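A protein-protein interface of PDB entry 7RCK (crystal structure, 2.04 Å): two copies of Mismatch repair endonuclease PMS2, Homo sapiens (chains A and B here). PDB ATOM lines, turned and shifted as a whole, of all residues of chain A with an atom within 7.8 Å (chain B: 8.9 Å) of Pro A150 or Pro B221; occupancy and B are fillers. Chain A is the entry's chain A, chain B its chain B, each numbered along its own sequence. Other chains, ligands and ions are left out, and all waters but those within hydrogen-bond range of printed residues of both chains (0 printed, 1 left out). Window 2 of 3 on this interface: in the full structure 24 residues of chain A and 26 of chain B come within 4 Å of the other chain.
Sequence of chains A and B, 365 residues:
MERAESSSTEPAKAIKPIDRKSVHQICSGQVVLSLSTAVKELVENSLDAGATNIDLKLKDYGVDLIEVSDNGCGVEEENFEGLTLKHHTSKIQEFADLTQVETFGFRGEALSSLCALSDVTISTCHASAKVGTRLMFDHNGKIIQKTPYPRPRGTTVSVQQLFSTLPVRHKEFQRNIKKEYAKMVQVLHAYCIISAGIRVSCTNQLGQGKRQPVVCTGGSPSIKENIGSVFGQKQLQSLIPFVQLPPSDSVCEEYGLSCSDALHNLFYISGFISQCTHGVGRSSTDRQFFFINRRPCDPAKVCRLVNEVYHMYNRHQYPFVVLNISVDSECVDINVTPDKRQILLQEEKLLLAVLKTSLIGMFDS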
ATOM      1  N   SER A 123      -3.473  12.783 -10.833  1.00  0.00           N
ATOM      2  CA  SER A 123      -3.512  11.521 -10.108  1.00  0.00           C
ATOM      3  C   SER A 123      -2.179  10.813 -10.309  1.00  0.00           C
ATOM      4  O   SER A 123      -1.622  10.827 -11.412  1.00  0.00           O
ATOM      5  CB  SER A 123      -4.661  10.627 -10.581  1.00  0.00           C
ATOM      6  OG  SER A 123      -4.376  10.045 -11.840  1.00  0.00           O
ATOM      7  N   THR A 124      -1.659  10.209  -9.245  1.00  0.00           N
ATOM      8  CA  THR A 124      -0.342   9.595  -9.324  1.00  0.00           C
ATOM      9  C   THR A 124      -0.243   8.472  -8.302  1.00  0.00           C
ATOM     10  O   THR A 124      -0.960   8.447  -7.299  1.00  0.00           O
ATOM     11  CB  THR A 124       0.770  10.630  -9.098  1.00  0.00           C
ATOM     12  OG1 THR A 124       2.046  10.041  -9.383  1.00  0.00           O
ATOM     13  CG2 THR A 124       0.756  11.127  -7.656  1.00  0.00           C
ATOM     14  N   CYS A 125       0.655   7.531  -8.581  1.00  0.00           N
ATOM     15  CA  CYS A 125       0.944   6.448  -7.649  1.00  0.00           C
ATOM     16  C   CYS A 125       2.393   6.028  -7.829  1.00  0.00           C
ATOM     17  O   CYS A 125       2.777   5.559  -8.905  1.00  0.00           O
ATOM     18  CB  CYS A 125       0.012   5.254  -7.859  1.00  0.00           C
ATOM     19  SG  CYS A 125       0.289   3.919  -6.666  1.00  0.00           S
ATOM     20  N   LYS A 130       0.936   2.258  -1.353  1.00  0.00           N
ATOM     21  CA  LYS A 130      -0.068   1.203  -1.401  1.00  0.00           C
ATOM     22  C   LYS A 130      -1.299   1.621  -2.189  1.00  0.00           C
ATOM     23  O   LYS A 130      -1.956   0.770  -2.799  1.00  0.00           O
ATOM     24  CB  LYS A 130      -0.479   0.792   0.016  1.00  0.00           C
ATOM     25  N   VAL A 131      -1.622   2.914  -2.186  1.00  0.00           N
ATOM     26  CA  VAL A 131      -2.721   3.457  -2.970  1.00  0.00           C
ATOM     27  C   VAL A 131      -2.282   4.796  -3.550  1.00  0.00           C
ATOM     28  O   VAL A 131      -1.475   5.518  -2.956  1.00  0.00           O
ATOM     29  CB  VAL A 131      -4.006   3.602  -2.115  1.00  0.00           C
ATOM     30  CG1 VAL A 131      -3.787   4.586  -0.973  1.00  0.00           C
ATOM     31  CG2 VAL A 131      -5.200   4.013  -2.969  1.00  0.00           C
ATOM     32  N   GLY A 132      -2.815   5.120  -4.723  1.00  0.00           N
ATOM     33  CA  GLY A 132      -2.525   6.380  -5.368  1.00  0.00           C
ATOM     34  C   GLY A 132      -3.264   7.537  -4.725  1.00  0.00           C
ATOM     35  O   GLY A 132      -4.021   7.387  -3.766  1.00  0.00           O
ATOM     36  N   THR A 133      -3.035   8.722  -5.285  1.00  0.00           N
ATOM     37  CA  THR A 133      -3.603   9.957  -4.767  1.00  0.00           C
ATOM     38  C   THR A 133      -4.058  10.827  -5.929  1.00  0.00           C
ATOM     39  O   THR A 133      -3.389  10.890  -6.964  1.00  0.00           O
ATOM     40  CB  THR A 133      -2.584  10.724  -3.910  1.00  0.00           C
ATOM     41  OG1 THR A 133      -2.066   9.859  -2.894  1.00  0.00           O
ATOM     42  CG2 THR A 133      -3.228  11.940  -3.256  1.00  0.00           C
ATOM     43  N   ARG A 134      -5.200  11.486  -5.755  1.00  0.00           N
ATOM     44  CA  ARG A 134      -5.733  12.428  -6.729  1.00  0.00           C
ATOM     45  C   ARG A 134      -5.638  13.833  -6.148  1.00  0.00           C
ATOM     46  O   ARG A 134      -6.077  14.069  -5.017  1.00  0.00           O
ATOM     47  CB  ARG A 134      -7.183  12.090  -7.083  1.00  0.00           C
ATOM     48  CG  ARG A 134      -7.786  12.960  -8.176  1.00  0.00           C
ATOM     49  CD  ARG A 134      -9.199  12.506  -8.507  1.00  0.00           C
ATOM     50  NE  ARG A 134      -9.772  13.241  -9.630  1.00  0.00           N
ATOM     51  CZ  ARG A 134     -10.421  14.393  -9.520  1.00  0.00           C
ATOM     52  NH1 ARG A 134     -10.583  14.987  -8.349  1.00  0.00           N
ATOM     53  NH2 ARG A 134     -10.919  14.963 -10.614  1.00  0.00           N
ATOM     54  N   THR A 147      -7.105  13.101  -2.163  1.00  0.00           N
ATOM     55  CA  THR A 147      -7.893  11.957  -1.741  1.00  0.00           C
ATOM     56  C   THR A 147      -7.224  10.671  -2.197  1.00  0.00           C
ATOM     57  O   THR A 147      -6.556  10.648  -3.236  1.00  0.00           O
ATOM     58  CB  THR A 147      -9.317  12.020  -2.318  1.00  0.00           C
ATOM     59  OG1 THR A 147      -9.256  11.972  -3.748  1.00  0.00           O
ATOM     60  CG2 THR A 147     -10.018  13.301  -1.891  1.00  0.00           C
ATOM     61  N   PRO A 148      -7.378   9.588  -1.434  1.00  0.00           N
ATOM     62  CA  PRO A 148      -6.885   8.288  -1.904  1.00  0.00           C
ATOM     63  C   PRO A 148      -7.551   7.909  -3.217  1.00  0.00           C
ATOM     64  O   PRO A 148      -8.748   8.129  -3.415  1.00  0.00           O
ATOM     65  CB  PRO A 148      -7.275   7.329  -0.773  1.00  0.00           C
ATOM     66  CG  PRO A 148      -7.384   8.201   0.436  1.00  0.00           C
ATOM     67  CD  PRO A 148      -7.911   9.516  -0.063  1.00  0.00           C
ATOM     68  N   TYR A 149      -6.765   7.336  -4.116  1.00  0.00           N
ATOM     69  CA  TYR A 149      -7.220   7.068  -5.479  1.00  0.00           C
ATOM     70  C   TYR A 149      -6.542   5.797  -5.962  1.00  0.00           C
ATOM     71  O   TYR A 149      -5.368   5.820  -6.363  1.00  0.00           O
ATOM     72  CB  TYR A 149      -6.897   8.250  -6.392  1.00  0.00           C
ATOM     73  CG  TYR A 149      -7.506   8.198  -7.773  1.00  0.00           C
ATOM     74  CD1 TYR A 149      -8.855   8.469  -7.970  1.00  0.00           C
ATOM     75  CD2 TYR A 149      -6.726   7.914  -8.886  1.00  0.00           C
ATOM     76  CE1 TYR A 149      -9.415   8.434  -9.234  1.00  0.00           C
ATOM     77  CE2 TYR A 149      -7.277   7.880 -10.155  1.00  0.00           C
ATOM     78  CZ  TYR A 149      -8.621   8.140 -10.323  1.00  0.00           C
ATOM     79  OH  TYR A 149      -9.174   8.104 -11.582  1.00  0.00           O
ATOM     80  N   PRO A 150      -7.248   4.665  -5.956  1.00  0.00           N
ATOM     81  CA  PRO A 150      -6.639   3.404  -6.408  1.00  0.00           C
ATOM     82  C   PRO A 150      -6.360   3.461  -7.902  1.00  0.00           C
ATOM     83  O   PRO A 150      -7.282   3.576  -8.713  1.00  0.00           O
ATOM     84  CB  PRO A 150      -7.698   2.350  -6.062  1.00  0.00           C
ATOM     85  CG  PRO A 150      -8.545   2.989  -5.004  1.00  0.00           C
ATOM     86  CD  PRO A 150      -8.576   4.449  -5.355  1.00  0.00           C
ATOM     87  N   ARG A 151      -5.083   3.388  -8.263  1.00  0.00           N
ATOM     88  CA  ARG A 151      -4.667   3.486  -9.653  1.00  0.00           C
ATOM     89  C   ARG A 151      -3.289   2.855  -9.787  1.00  0.00           C
ATOM     90  O   ARG A 151      -2.547   2.761  -8.802  1.00  0.00           O
ATOM     91  CB  ARG A 151      -4.648   4.949 -10.127  1.00  0.00           C
ATOM     92  CG  ARG A 151      -3.688   5.853  -9.368  1.00  0.00           C
ATOM     93  CD  ARG A 151      -3.151   6.950 -10.277  1.00  0.00           C
ATOM     94  NE  ARG A 151      -2.289   6.401 -11.317  1.00  0.00           N
ATOM     95  CZ  ARG A 151      -2.106   6.951 -12.509  1.00  0.00           C
ATOM     96  NH1 ARG A 151      -2.726   8.066 -12.859  1.00  0.00           N
ATOM     97  NH2 ARG A 151      -1.285   6.361 -13.376  1.00  0.00           N
ATOM     98  N   PRO A 152      -2.925   2.396 -10.983  1.00  0.00           N
ATOM     99  CA  PRO A 152      -1.602   1.789 -11.171  1.00  0.00           C
ATOM    100  C   PRO A 152      -0.489   2.828 -11.123  1.00  0.00           C
ATOM    101  O   PRO A 152      -0.715   4.041 -11.138  1.00  0.00           O
ATOM    102  CB  PRO A 152      -1.701   1.138 -12.553  1.00  0.00           C
ATOM    103  CG  PRO A 152      -2.776   1.899 -13.254  1.00  0.00           C
ATOM    104  CD  PRO A 152      -3.761   2.285 -12.191  1.00  0.00           C
ATOM    105  N   ILE B 193     -14.323  -2.105 -19.639  1.00  0.00           N
ATOM    106  CA  ILE B 193     -15.272  -1.584 -18.661  1.00  0.00           C
ATOM    107  C   ILE B 193     -14.995  -2.164 -17.278  1.00  0.00           C
ATOM    108  O   ILE B 193     -14.964  -1.438 -16.278  1.00  0.00           O
ATOM    109  CB  ILE B 193     -16.714  -1.875 -19.117  1.00  0.00           C
ATOM    110  CG1 ILE B 193     -17.073  -1.020 -20.334  1.00  0.00           C
ATOM    111  CG2 ILE B 193     -17.698  -1.642 -17.982  1.00  0.00           C
ATOM    112  CD1 ILE B 193     -18.359  -1.438 -21.015  1.00  0.00           C
ATOM    113  N   ILE B 194     -14.785  -3.480 -17.200  1.00  0.00           N
ATOM    114  CA  ILE B 194     -14.720  -4.159 -15.910  1.00  0.00           C
ATOM    115  C   ILE B 194     -13.334  -4.137 -15.269  1.00  0.00           C
ATOM    116  O   ILE B 194     -13.225  -4.339 -14.050  1.00  0.00           O
ATOM    117  CB  ILE B 194     -15.211  -5.613 -16.050  1.00  0.00           C
ATOM    118  CG1 ILE B 194     -15.662  -6.165 -14.696  1.00  0.00           C
ATOM    119  CG2 ILE B 194     -14.131  -6.494 -16.664  1.00  0.00           C
ATOM    120  CD1 ILE B 194     -16.884  -5.468 -14.131  1.00  0.00           C
ATOM    121  N   SER B 195     -12.275  -3.889 -16.041  1.00  0.00           N
ATOM    122  CA  SER B 195     -10.909  -3.971 -15.516  1.00  0.00           C
ATOM    123  C   SER B 195     -10.509  -2.634 -14.889  1.00  0.00           C
ATOM    124  O   SER B 195      -9.703  -1.866 -15.417  1.00  0.00           O
ATOM    125  CB  SER B 195      -9.939  -4.392 -16.612  1.00  0.00           C
ATOM    126  OG  SER B 195     -10.320  -5.635 -17.177  1.00  0.00           O
ATOM    127  N   ALA B 196     -11.100  -2.369 -13.725  1.00  0.00           N
ATOM    128  CA  ALA B 196     -10.750  -1.179 -12.965  1.00  0.00           C
ATOM    129  C   ALA B 196      -9.301  -1.254 -12.500  1.00  0.00           C
ATOM    130  O   ALA B 196      -8.814  -2.314 -12.096  1.00  0.00           O
ATOM    131  CB  ALA B 196     -11.683  -1.022 -11.764  1.00  0.00           C
ATOM    132  N   GLY B 197      -8.606  -0.121 -12.570  1.00  0.00           N
ATOM    133  CA  GLY B 197      -7.211  -0.072 -12.189  1.00  0.00           C
ATOM    134  C   GLY B 197      -6.250  -0.593 -13.232  1.00  0.00           C
ATOM    135  O   GLY B 197      -5.044  -0.666 -12.960  1.00  0.00           O
ATOM    136  N   ILE B 198      -6.740  -0.972 -14.408  1.00  0.00           N
ATOM    137  CA  ILE B 198      -5.917  -1.527 -15.474  1.00  0.00           C
ATOM    138  C   ILE B 198      -6.101  -0.674 -16.719  1.00  0.00           C
ATOM    139  O   ILE B 198      -7.235  -0.405 -17.132  1.00  0.00           O
ATOM    140  CB  ILE B 198      -6.274  -2.994 -15.763  1.00  0.00           C
ATOM    141  CG1 ILE B 198      -6.110  -3.829 -14.495  1.00  0.00           C
ATOM    142  CG2 ILE B 198      -5.407  -3.543 -16.888  1.00  0.00           C
ATOM    143  CD1 ILE B 198      -6.704  -5.205 -14.581  1.00  0.00           C
ATOM    144  N   GLY B 218      -7.926   4.733 -18.697  1.00  0.00           N
ATOM    145  CA  GLY B 218      -6.984   5.504 -17.915  1.00  0.00           C
ATOM    146  C   GLY B 218      -6.565   4.899 -16.594  1.00  0.00           C
ATOM    147  O   GLY B 218      -5.966   5.609 -15.778  1.00  0.00           O
ATOM    148  N   GLY B 219      -6.836   3.621 -16.359  1.00  0.00           N
ATOM    149  CA  GLY B 219      -6.490   3.017 -15.088  1.00  0.00           C
ATOM    150  C   GLY B 219      -7.321   3.531 -13.934  1.00  0.00           C
ATOM    151  O   GLY B 219      -6.803   3.680 -12.819  1.00  0.00           O
ATOM    152  N   SER B 220      -8.599   3.802 -14.171  1.00  0.00           N
ATOM    153  CA  SER B 220      -9.472   4.382 -13.166  1.00  0.00           C
ATOM    154  C   SER B 220     -10.066   3.297 -12.270  1.00  0.00           C
ATOM    155  O   SER B 220     -10.300   2.171 -12.715  1.00  0.00           O
ATOM    156  CB  SER B 220     -10.596   5.168 -13.833  1.00  0.00           C
ATOM    157  OG  SER B 220     -11.529   5.628 -12.872  1.00  0.00           O
ATOM    158  N   PRO B 221     -10.315   3.615 -10.997  1.00  0.00           N
ATOM    159  CA  PRO B 221     -10.869   2.617 -10.075  1.00  0.00           C
ATOM    160  C   PRO B 221     -12.369   2.405 -10.197  1.00  0.00           C
ATOM    161  O   PRO B 221     -12.905   1.531  -9.507  1.00  0.00           O
ATOM    162  CB  PRO B 221     -10.512   3.194  -8.698  1.00  0.00           C
ATOM    163  CG  PRO B 221     -10.498   4.666  -8.914  1.00  0.00           C
ATOM    164  CD  PRO B 221      -9.958   4.868 -10.306  1.00  0.00           C
ATOM    165  N   SER B 222     -13.070   3.158 -11.040  1.00  0.00           N
ATOM    166  CA  SER B 222     -14.520   3.065 -11.120  1.00  0.00           C
ATOM    167  C   SER B 222     -14.946   2.598 -12.504  1.00  0.00           C
ATOM    168  O   SER B 222     -14.363   3.000 -13.517  1.00  0.00           O
ATOM    169  CB  SER B 222     -15.181   4.411 -10.800  1.00  0.00           C
ATOM    170  OG  SER B 222     -15.234   5.240 -11.948  1.00  0.00           O
ATOM    171  N   ILE B 223     -15.979   1.752 -12.532  1.00  0.00           N
ATOM    172  CA  ILE B 223     -16.571   1.317 -13.792  1.00  0.00           C
ATOM    173  C   ILE B 223     -17.138   2.502 -14.560  1.00  0.00           C
ATOM    174  O   ILE B 223     -17.097   2.529 -15.797  1.00  0.00           O
ATOM    175  CB  ILE B 223     -17.642   0.241 -13.518  1.00  0.00           C
ATOM    176  CG1 ILE B 223     -16.988  -1.036 -12.984  1.00  0.00           C
ATOM    177  CG2 ILE B 223     -18.463  -0.057 -14.766  1.00  0.00           C
ATOM    178  CD1 ILE B 223     -17.977  -2.071 -12.500  1.00  0.00           C
ATOM    179  N   LYS B 224     -17.662   3.504 -13.849  1.00  0.00           N
ATOM    180  CA  LYS B 224     -18.256   4.658 -14.516  1.00  0.00           C
ATOM    181  C   LYS B 224     -17.233   5.397 -15.372  1.00  0.00           C
ATOM    182  O   LYS B 224     -17.523   5.766 -16.517  1.00  0.00           O
ATOM    183  CB  LYS B 224     -18.879   5.596 -13.482  1.00  0.00           C
ATOM    184  CG  LYS B 224     -19.603   6.792 -14.081  1.00  0.00           C
ATOM    185  CD  LYS B 224     -20.301   7.608 -13.003  1.00  0.00           C
ATOM    186  CE  LYS B 224     -21.032   8.798 -13.602  1.00  0.00           C
ATOM    187  NZ  LYS B 224     -21.720   9.613 -12.561  1.00  0.00           N
ATOM    188  N   GLU B 225     -16.026   5.616 -14.843  1.00  0.00           N
ATOM    189  CA  GLU B 225     -15.005   6.295 -15.635  1.00  0.00           C
ATOM    190  C   GLU B 225     -14.508   5.416 -16.776  1.00  0.00           C
ATOM    191  O   GLU B 225     -14.179   5.930 -17.851  1.00  0.00           O
ATOM    192  CB  GLU B 225     -13.836   6.734 -14.754  1.00  0.00           C
ATOM    193  CG  GLU B 225     -14.182   7.820 -13.749  1.00  0.00           C
ATOM    194  CD  GLU B 225     -12.971   8.297 -12.966  1.00  0.00           C
ATOM    195  OE1 GLU B 225     -11.918   8.545 -13.590  1.00  0.00           O
ATOM    196  OE2 GLU B 225     -13.072   8.427 -11.727  1.00  0.00           O
ATOM    197  N   ASN B 226     -14.439   4.099 -16.563  1.00  0.00           N
ATOM    198  CA  ASN B 226     -14.073   3.203 -17.654  1.00  0.00           C
ATOM    199  C   ASN B 226     -15.100   3.266 -18.776  1.00  0.00           C
ATOM    200  O   ASN B 226     -14.739   3.246 -19.959  1.00  0.00           O
ATOM    201  CB  ASN B 226     -13.922   1.772 -17.134  1.00  0.00           C
ATOM    202  CG  ASN B 226     -12.622   1.561 -16.384  1.00  0.00           C
ATOM    203  OD1 ASN B 226     -11.661   2.309 -16.561  1.00  0.00           O
ATOM    204  ND2 ASN B 226     -12.585   0.538 -15.540  1.00  0.00           N
ATOM    205  N   ARG B 294     -17.223 -10.468 -12.210  1.00  0.00           N
ATOM    206  CA  ARG B 294     -16.333  -9.671 -13.054  1.00  0.00           C
ATOM    207  C   ARG B 294     -15.974 -10.353 -14.370  1.00  0.00           C
ATOM    208  O   ARG B 294     -15.184  -9.793 -15.140  1.00  0.00           O
ATOM    209  CB  ARG B 294     -15.027  -9.286 -12.339  1.00  0.00           C
ATOM    210  CG  ARG B 294     -15.171  -8.945 -10.861  1.00  0.00           C
ATOM    211  CD  ARG B 294     -15.806  -7.586 -10.636  1.00  0.00           C
ATOM    212  NE  ARG B 294     -14.993  -6.499 -11.169  1.00  0.00           N
ATOM    213  CZ  ARG B 294     -15.151  -5.223 -10.845  1.00  0.00           C
ATOM    214  NH1 ARG B 294     -16.061  -4.842  -9.963  1.00  0.00           N
ATOM    215  NH2 ARG B 294     -14.376  -4.306 -11.417  1.00  0.00           N
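OH of Tyr A149 sits at hydrogen-bond distance from OE1 of Glu B225.
The side-chain hydroxyl of Ser A123 lies within hydrogen-bond range of the guanidinium group of Arg A151, at 2.8 Å.
The backbone carbonyl oxygen of Arg A151 lies close to the side-chain sulfur of Cys A125 (3.7 Å).
The side-chain hydroxyl (OG) of Ser B220 lies close to the backbone NH (N) of Ser B222 (3.4 Å).
The side-chain hydroxyl (OG) of Ser B222 sits at hydrogen-bond distance from the backbone NH (N) of Glu B225 (3.0 Å).
N of Tyr A149 sits at hydrogen-bond distance from O of Gly A132 (2.8 Å).
OE1 of Glu B225 sits at hydrogen-bond distance from OG of Ser B220, at 3.0 Å.
OH of Tyr A149 touches OG of Ser B220, 3.7 Å away.
Pro B221 touches Tyr A149 (CD to CZ, 3.5 Å).
O of Pro A150 touches CB of Pro B221, at 3.3 Å.
Arg A151 touches Gly B219 (CB to O, 3.7 Å).
CD of Pro A152 touches O of Gly B197 (3.3 Å).
O of Gly B219 touches CD of Pro A152, at 3.4 Å.
Of chain B, only Pro B221 comes within 4 Å of Pro A150.
Pro B221 touches just these residues of chain A: Tyr A149 and Pro A150.
Tyr A149 touches just these residues of chain B: Ser B220 (3.7 Å), Pro B221 (3.5 Å) and Glu B225 (3.4 Å).
Ser B220 touches one residue of chain A.
Printed residues of chain A within 4 Å of Gly B219: Arg A151 and Pro A152.
Of the printed residues of chain A, Gly B197 touches Pro A152 (3.3 Å).
Lys A130 touches none of the printed residues of chain B.
Ile B193 touches none of the printed residues of chain A.
Of the 14 printed residues of chain A, 4 touch a printed residue of chain B.
Of the 16 printed residues of chain B, 5 touch a printed residue of chain A.
Hydrophobic or aromatic side chains of chain B that line the printed part of chain A: Pro B221.
No position is printed for both chains.
Of the 7 pairs that touch across the chains among the printed residues, none has its exchanged pair printed and touching as well.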
